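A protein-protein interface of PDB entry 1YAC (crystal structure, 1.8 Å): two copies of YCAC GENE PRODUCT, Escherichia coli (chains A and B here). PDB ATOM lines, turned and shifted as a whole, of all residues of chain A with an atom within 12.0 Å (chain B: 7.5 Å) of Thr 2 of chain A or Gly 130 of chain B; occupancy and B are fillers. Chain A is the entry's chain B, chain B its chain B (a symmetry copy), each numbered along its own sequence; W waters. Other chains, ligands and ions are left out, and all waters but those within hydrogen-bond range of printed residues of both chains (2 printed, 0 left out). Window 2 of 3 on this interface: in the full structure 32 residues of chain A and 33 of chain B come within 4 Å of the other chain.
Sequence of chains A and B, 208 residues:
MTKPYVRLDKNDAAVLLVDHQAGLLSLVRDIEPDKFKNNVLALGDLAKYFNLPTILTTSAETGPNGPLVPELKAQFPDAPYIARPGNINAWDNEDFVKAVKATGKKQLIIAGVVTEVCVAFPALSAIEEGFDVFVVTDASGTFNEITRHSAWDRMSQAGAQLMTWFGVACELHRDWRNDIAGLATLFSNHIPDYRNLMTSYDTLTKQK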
ATOM      1  N   THR A   2      12.700   7.529 -11.015  1.00  0.00           N
ATOM      2  CA  THR A   2      12.905   8.535 -12.078  1.00  0.00           C
ATOM      3  C   THR A   2      12.769   7.774 -13.401  1.00  0.00           C
ATOM      4  O   THR A   2      11.827   6.996 -13.563  1.00  0.00           O
ATOM      5  CB  THR A   2      14.313   9.150 -11.968  1.00  0.00           C
ATOM      6  OG1 THR A   2      14.624   9.346 -10.574  1.00  0.00           O
ATOM      7  CG2 THR A   2      14.397  10.472 -12.714  1.00  0.00           C
ATOM      8  N   LYS A   3      13.680   8.002 -14.345  1.00  0.00           N
ATOM      9  CA  LYS A   3      13.632   7.268 -15.590  1.00  0.00           C
ATOM     10  C   LYS A   3      14.130   5.879 -15.247  1.00  0.00           C
ATOM     11  O   LYS A   3      15.146   5.735 -14.567  1.00  0.00           O
ATOM     12  CB  LYS A   3      14.530   7.907 -16.641  1.00  0.00           C
ATOM     13  CG  LYS A   3      14.053   9.269 -17.077  1.00  0.00           C
ATOM     14  CD  LYS A   3      14.166   9.426 -18.576  1.00  0.00           C
ATOM     15  CE  LYS A   3      13.735  10.818 -19.001  1.00  0.00           C
ATOM     16  NZ  LYS A   3      13.945  11.045 -20.460  1.00  0.00           N
ATOM     17  N   PRO A   4      13.360   4.847 -15.609  1.00  0.00           N
ATOM     18  CA  PRO A   4      13.756   3.470 -15.327  1.00  0.00           C
ATOM     19  C   PRO A   4      14.925   3.073 -16.214  1.00  0.00           C
ATOM     20  O   PRO A   4      15.025   3.515 -17.359  1.00  0.00           O
ATOM     21  CB  PRO A   4      12.514   2.662 -15.716  1.00  0.00           C
ATOM     22  CG  PRO A   4      11.403   3.650 -15.634  1.00  0.00           C
ATOM     23  CD  PRO A   4      12.018   4.889 -16.205  1.00  0.00           C
ATOM     24  N   TYR A   5      15.801   2.237 -15.676  1.00  0.00           N
ATOM     25  CA  TYR A   5      16.944   1.732 -16.417  1.00  0.00           C
ATOM     26  C   TYR A   5      16.407   0.522 -17.186  1.00  0.00           C
ATOM     27  O   TYR A   5      16.198  -0.550 -16.616  1.00  0.00           O
ATOM     28  CB  TYR A   5      18.036   1.343 -15.414  1.00  0.00           C
ATOM     29  CG  TYR A   5      19.286   0.675 -15.949  1.00  0.00           C
ATOM     30  CD1 TYR A   5      19.598   0.656 -17.309  1.00  0.00           C
ATOM     31  CD2 TYR A   5      20.153   0.043 -15.070  1.00  0.00           C
ATOM     32  CE1 TYR A   5      20.750   0.009 -17.768  1.00  0.00           C
ATOM     33  CE2 TYR A   5      21.290  -0.597 -15.505  1.00  0.00           C
ATOM     34  CZ  TYR A   5      21.588  -0.622 -16.851  1.00  0.00           C
ATOM     35  OH  TYR A   5      22.700  -1.339 -17.247  1.00  0.00           O
ATOM     36  N   VAL A   6      16.113   0.719 -18.463  1.00  0.00           N
ATOM     37  CA  VAL A   6      15.582  -0.348 -19.311  1.00  0.00           C
ATOM     38  C   VAL A   6      16.771  -1.135 -19.829  1.00  0.00           C
ATOM     39  O   VAL A   6      17.307  -0.834 -20.903  1.00  0.00           O
ATOM     40  CB  VAL A   6      14.740   0.239 -20.488  1.00  0.00           C
ATOM     41  CG1 VAL A   6      14.185  -0.881 -21.388  1.00  0.00           C
ATOM     42  CG2 VAL A   6      13.587   1.057 -19.926  1.00  0.00           C
ATOM     43  N   ARG A   7      17.203  -2.122 -19.049  1.00  0.00           N
ATOM     44  CA  ARG A   7      18.370  -2.902 -19.430  1.00  0.00           C
ATOM     45  C   ARG A   7      18.122  -4.216 -20.128  1.00  0.00           C
ATOM     46  O   ARG A   7      17.070  -4.840 -19.960  1.00  0.00           O
ATOM     47  CB  ARG A   7      19.320  -3.089 -18.247  1.00  0.00           C
ATOM     48  CG  ARG A   7      18.768  -3.817 -17.079  1.00  0.00           C
ATOM     49  CD  ARG A   7      19.895  -4.098 -16.111  1.00  0.00           C
ATOM     50  NE  ARG A   7      19.417  -4.580 -14.824  1.00  0.00           N
ATOM     51  CZ  ARG A   7      20.220  -4.949 -13.830  1.00  0.00           C
ATOM     52  NH1 ARG A   7      21.542  -4.890 -13.978  1.00  0.00           N
ATOM     53  NH2 ARG A   7      19.703  -5.409 -12.702  1.00  0.00           N
ATOM     54  N   TRP B  91      26.124  -1.672  -9.235  1.00  0.00           N
ATOM     55  CA  TRP B  91      24.855  -1.525  -8.532  1.00  0.00           C
ATOM     56  C   TRP B  91      24.225  -2.884  -8.215  1.00  0.00           C
ATOM     57  O   TRP B  91      23.371  -2.975  -7.335  1.00  0.00           O
ATOM     58  CB  TRP B  91      23.886  -0.652  -9.333  1.00  0.00           C
ATOM     59  CG  TRP B  91      22.925   0.134  -8.458  1.00  0.00           C
ATOM     60  CD1 TRP B  91      21.632  -0.200  -8.141  1.00  0.00           C
ATOM     61  CD2 TRP B  91      23.192   1.376  -7.790  1.00  0.00           C
ATOM     62  NE1 TRP B  91      21.084   0.757  -7.320  1.00  0.00           N
ATOM     63  CE2 TRP B  91      22.018   1.736  -7.090  1.00  0.00           C
ATOM     64  CE3 TRP B  91      24.317   2.219  -7.713  1.00  0.00           C
ATOM     65  CZ2 TRP B  91      21.929   2.907  -6.323  1.00  0.00           C
ATOM     66  CZ3 TRP B  91      24.231   3.382  -6.955  1.00  0.00           C
ATOM     67  CH2 TRP B  91      23.043   3.714  -6.270  1.00  0.00           C
ATOM     68  N   LYS B 106      22.829  12.568  -1.796  1.00  0.00           N
ATOM     69  CA  LYS B 106      21.860  12.537  -2.892  1.00  0.00           C
ATOM     70  C   LYS B 106      22.577  12.577  -4.248  1.00  0.00           C
ATOM     71  O   LYS B 106      22.105  12.000  -5.235  1.00  0.00           O
ATOM     72  CB  LYS B 106      20.959  13.776  -2.799  1.00  0.00           C
ATOM     73  CG  LYS B 106      19.479  13.592  -3.150  1.00  0.00           C
ATOM     74  CD  LYS B 106      19.224  13.228  -4.568  1.00  0.00           C
ATOM     75  CE  LYS B 106      17.766  13.449  -4.922  1.00  0.00           C
ATOM     76  NZ  LYS B 106      16.879  12.341  -4.447  1.00  0.00           N
ATOM     77  N   GLN B 107      23.687  13.303  -4.300  1.00  0.00           N
ATOM     78  CA  GLN B 107      24.438  13.451  -5.545  1.00  0.00           C
ATOM     79  C   GLN B 107      25.576  12.457  -5.647  1.00  0.00           C
ATOM     80  O   GLN B 107      26.329  12.274  -4.683  1.00  0.00           O
ATOM     81  CB  GLN B 107      24.992  14.866  -5.642  1.00  0.00           C
ATOM     82  CG  GLN B 107      23.934  15.941  -5.480  1.00  0.00           C
ATOM     83  CD  GLN B 107      24.533  17.328  -5.487  1.00  0.00           C
ATOM     84  OE1 GLN B 107      25.702  17.509  -5.150  1.00  0.00           O
ATOM     85  NE2 GLN B 107      23.737  18.315  -5.868  1.00  0.00           N
ATOM     86  N   LEU B 124      22.879   4.590 -14.602  1.00  0.00           N
ATOM     87  CA  LEU B 124      21.484   4.371 -14.990  1.00  0.00           C
ATOM     88  C   LEU B 124      20.684   3.768 -13.837  1.00  0.00           C
ATOM     89  O   LEU B 124      19.523   4.132 -13.623  1.00  0.00           O
ATOM     90  CB  LEU B 124      21.401   3.481 -16.237  1.00  0.00           C
ATOM     91  CG  LEU B 124      22.016   4.114 -17.496  1.00  0.00           C
ATOM     92  CD1 LEU B 124      22.108   3.098 -18.638  1.00  0.00           C
ATOM     93  CD2 LEU B 124      21.208   5.317 -17.919  1.00  0.00           C
ATOM     94  N   SER B 125      21.303   2.846 -13.107  1.00  0.00           N
ATOM     95  CA  SER B 125      20.660   2.216 -11.950  1.00  0.00           C
ATOM     96  C   SER B 125      20.375   3.266 -10.878  1.00  0.00           C
ATOM     97  O   SER B 125      19.271   3.323 -10.320  1.00  0.00           O
ATOM     98  CB  SER B 125      21.568   1.141 -11.349  1.00  0.00           C
ATOM     99  OG  SER B 125      21.644   0.000 -12.177  1.00  0.00           O
ATOM    100  N   ALA B 126      21.368   4.115 -10.625  1.00  0.00           N
ATOM    101  CA  ALA B 126      21.259   5.155  -9.608  1.00  0.00           C
ATOM    102  C   ALA B 126      20.177   6.171  -9.948  1.00  0.00           C
ATOM    103  O   ALA B 126      19.423   6.608  -9.066  1.00  0.00           O
ATOM    104  CB  ALA B 126      22.611   5.838  -9.401  1.00  0.00           C
ATOM    105  N   ILE B 127      20.080   6.525 -11.228  1.00  0.00           N
ATOM    106  CA  ILE B 127      19.066   7.471 -11.678  1.00  0.00           C
ATOM    107  C   ILE B 127      17.691   6.881 -11.419  1.00  0.00           C
ATOM    108  O   ILE B 127      16.798   7.579 -10.935  1.00  0.00           O
ATOM    109  CB  ILE B 127      19.221   7.809 -13.186  1.00  0.00           C
ATOM    110  CG1 ILE B 127      20.410   8.761 -13.376  1.00  0.00           C
ATOM    111  CG2 ILE B 127      17.920   8.436 -13.756  1.00  0.00           C
ATOM    112  CD1 ILE B 127      20.810   8.983 -14.835  1.00  0.00           C
ATOM    113  N   GLU B 128      17.532   5.591 -11.696  1.00  0.00           N
ATOM    114  CA  GLU B 128      16.247   4.941 -11.461  1.00  0.00           C
ATOM    115  C   GLU B 128      15.898   5.017  -9.978  1.00  0.00           C
ATOM    116  O   GLU B 128      14.742   5.251  -9.622  1.00  0.00           O
ATOM    117  CB  GLU B 128      16.260   3.478 -11.909  1.00  0.00           C
ATOM    118  CG  GLU B 128      14.968   2.751 -11.564  1.00  0.00           C
ATOM    119  CD  GLU B 128      14.898   1.346 -12.117  1.00  0.00           C
ATOM    120  OE1 GLU B 128      15.478   1.090 -13.185  1.00  0.00           O
ATOM    121  OE2 GLU B 128      14.234   0.494 -11.492  1.00  0.00           O
ATOM    122  N   GLU B 129      16.911   4.872  -9.128  1.00  0.00           N
ATOM    123  CA  GLU B 129      16.718   4.919  -7.686  1.00  0.00           C
ATOM    124  C   GLU B 129      16.480   6.315  -7.121  1.00  0.00           C
ATOM    125  O   GLU B 129      16.246   6.460  -5.926  1.00  0.00           O
ATOM    126  CB  GLU B 129      17.866   4.223  -6.951  1.00  0.00           C
ATOM    127  CG  GLU B 129      17.905   2.727  -7.187  1.00  0.00           C
ATOM    128  CD  GLU B 129      18.074   1.916  -5.916  1.00  0.00           C
ATOM    129  OE1 GLU B 129      17.793   2.445  -4.816  1.00  0.00           O
ATOM    130  OE2 GLU B 129      18.470   0.732  -6.018  1.00  0.00           O
ATOM    131  N   GLY B 130      16.552   7.337  -7.967  1.00  0.00           N
ATOM    132  CA  GLY B 130      16.295   8.692  -7.505  1.00  0.00           C
ATOM    133  C   GLY B 130      17.476   9.601  -7.234  1.00  0.00           C
ATOM    134  O   GLY B 130      17.289  10.768  -6.871  1.00  0.00           O
ATOM    135  N   PHE B 131      18.689   9.095  -7.438  1.00  0.00           N
ATOM    136  CA  PHE B 131      19.890   9.891  -7.196  1.00  0.00           C
ATOM    137  C   PHE B 131      20.162  10.911  -8.304  1.00  0.00           C
ATOM    138  O   PHE B 131      19.708  10.756  -9.436  1.00  0.00           O
ATOM    139  CB  PHE B 131      21.116   8.970  -7.069  1.00  0.00           C
ATOM    140  CG  PHE B 131      21.137   8.139  -5.820  1.00  0.00           C
ATOM    141  CD1 PHE B 131      21.738   8.624  -4.662  1.00  0.00           C
ATOM    142  CD2 PHE B 131      20.605   6.852  -5.812  1.00  0.00           C
ATOM    143  CE1 PHE B 131      21.819   7.824  -3.510  1.00  0.00           C
ATOM    144  CE2 PHE B 131      20.678   6.049  -4.672  1.00  0.00           C
ATOM    145  CZ  PHE B 131      21.290   6.542  -3.520  1.00  0.00           C
ATOM    146  N   ASP B 132      20.891  11.964  -7.969  1.00  0.00           N
ATOM    147  CA  ASP B 132      21.281  12.968  -8.964  1.00  0.00           C
ATOM    148  C   ASP B 132      22.682  12.541  -9.395  1.00  0.00           C
ATOM    149  O   ASP B 132      23.621  12.570  -8.606  1.00  0.00           O
ATOM    150  CB  ASP B 132      21.276  14.367  -8.362  1.00  0.00           C
ATOM    151  CG  ASP B 132      19.881  14.846  -8.064  1.00  0.00           C
ATOM    152  OD1 ASP B 132      18.986  14.519  -8.865  1.00  0.00           O
ATOM    153  OD2 ASP B 132      19.674  15.507  -7.029  1.00  0.00           O
ATOM    154  N   VAL B 133      22.789  12.096 -10.644  1.00  0.00           N
ATOM    155  CA  VAL B 133      24.045  11.585 -11.174  1.00  0.00           C
ATOM    156  C   VAL B 133      24.824  12.572 -12.043  1.00  0.00           C
ATOM    157  O   VAL B 133      24.282  13.205 -12.954  1.00  0.00           O
ATOM    158  CB  VAL B 133      23.802  10.253 -11.936  1.00  0.00           C
ATOM    159  CG1 VAL B 133      25.119   9.689 -12.454  1.00  0.00           C
ATOM    160  CG2 VAL B 133      23.095   9.237 -11.021  1.00  0.00           C
ATOM    161  N   ALA B 158      18.943   9.480 -20.062  1.00  0.00           N
ATOM    162  CA  ALA B 158      18.359   9.080 -18.775  1.00  0.00           C
ATOM    163  C   ALA B 158      18.298  10.206 -17.755  1.00  0.00           C
ATOM    164  O   ALA B 158      17.631  10.065 -16.732  1.00  0.00           O
ATOM    165  CB  ALA B 158      19.135   7.907 -18.189  1.00  0.00           C
ATOM    166  N   GLY B 159      19.028  11.291 -18.001  1.00  0.00           N
ATOM    167  CA  GLY B 159      19.035  12.407 -17.076  1.00  0.00           C
ATOM    168  C   GLY B 159      20.353  12.669 -16.357  1.00  0.00           C
ATOM    169  O   GLY B 159      20.419  13.551 -15.495  1.00  0.00           O
HETATM  170  O   HOH W   1      17.129  10.277 -10.488  1.00  0.00           O
HETATM  171  O   HOH W   2      17.888   5.296 -15.577  1.00  0.00           O
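The backbone carbonyl oxygen of Gly 130 of chain B sits at hydrogen-bond distance from the side-chain amino group of Lys 106 of chain B (2.9 Å).
Water W1 lies within hydrogen-bond range of OG1 of Thr 2 of chain A (2.7 Å), O of Ile 127 of chain B (2.8 Å) and O of Phe 131 of chain B (2.8 Å).
Water W2 lies within hydrogen-bond range of the backbone carbonyl oxygen (O) of Leu 124 of chain B (2.8 Å) and the backbone carbonyl oxygen (O) of Lys 3 of chain A (3.0 Å).
O of Glu 128 of chain B lies within hydrogen-bond range of N of Thr 2 of chain A, 3.4 Å away.
The backbone NH (N) of Tyr 5 of chain A is in hydrogen-bond range of the side-chain carboxylate (OE1) of Glu 128 of chain B, 2.8 Å away.
The side-chain hydroxyl of Thr 2 of chain A sits at hydrogen-bond distance from the backbone carbonyl oxygen of Ile 127 of chain B (2.8 Å).
Printed residues of chain B within 4 Å of Thr 2 of chain A: Ile 127 (2.8 Å), Glu 128 (3.4 Å) and Gly 130 (3.6 Å).
Gly 130 of chain B touches just one residue of chain A: Thr 2 (3.6 Å).
Ile 127 of chain B touches just these residues of chain A: Thr 2 and Lys 3.
Glu 128 of chain B touches four residues of chain A.
No residue of chain A comes within 4 Å of Asp 132 of chain B.
No residue of chain A comes within 4 Å of Gly 159 of chain B.
Of the printed residues of chain A, Ala 158 of chain B touches Lys 3 (3.7 Å).
Printed residues of chain B within 4 Å of Tyr 5 of chain A: Leu 124, Ser 125 and Glu 128.
Printed residues of chain A within 4 Å of Leu 124 of chain B: Tyr 5.
Val 133 of chain B touches none of the printed residues of chain A.
Hydrophobic or aromatic side chains of chain A that line the printed part of chain B: Tyr 5.
Along chain A the printed residues that touch a printed residue of chain B span positions 2 to 5.
Of the 15 printed residues of chain B, 6 touch a printed residue of chain A.
Printed residues of chain B that touch a printed residue of chain A: Leu 124, Ser 125, Ile 127, Glu 128, Gly 130 and Ala 158.
Hydrophobic or aromatic side chains of chain B within 4 Å of the printed part of chain A: Leu 124 and Ile 127.
Among the printed residues, 10 pairs touch across the chains.
Among the printed residues, merely in contact across the chains: Tyr 5 of chain A with Ser 125 of chain B, Lys 3 of chain A with Glu 128 of chain B, Tyr 5 of chain A with Leu 124 of chain B, Thr 2 of chain A with Gly 130 of chain B, Pro 4 of chain A with Glu 128 of chain B, Lys 3 of chain A with Ala 158 of chain B and Lys 3 of chain A with Ile 127 of chain B.
No position is printed for both chains.
Of the 10 pairs that touch across the chains among the printed residues, none has its exchanged pair printed and touching as well.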
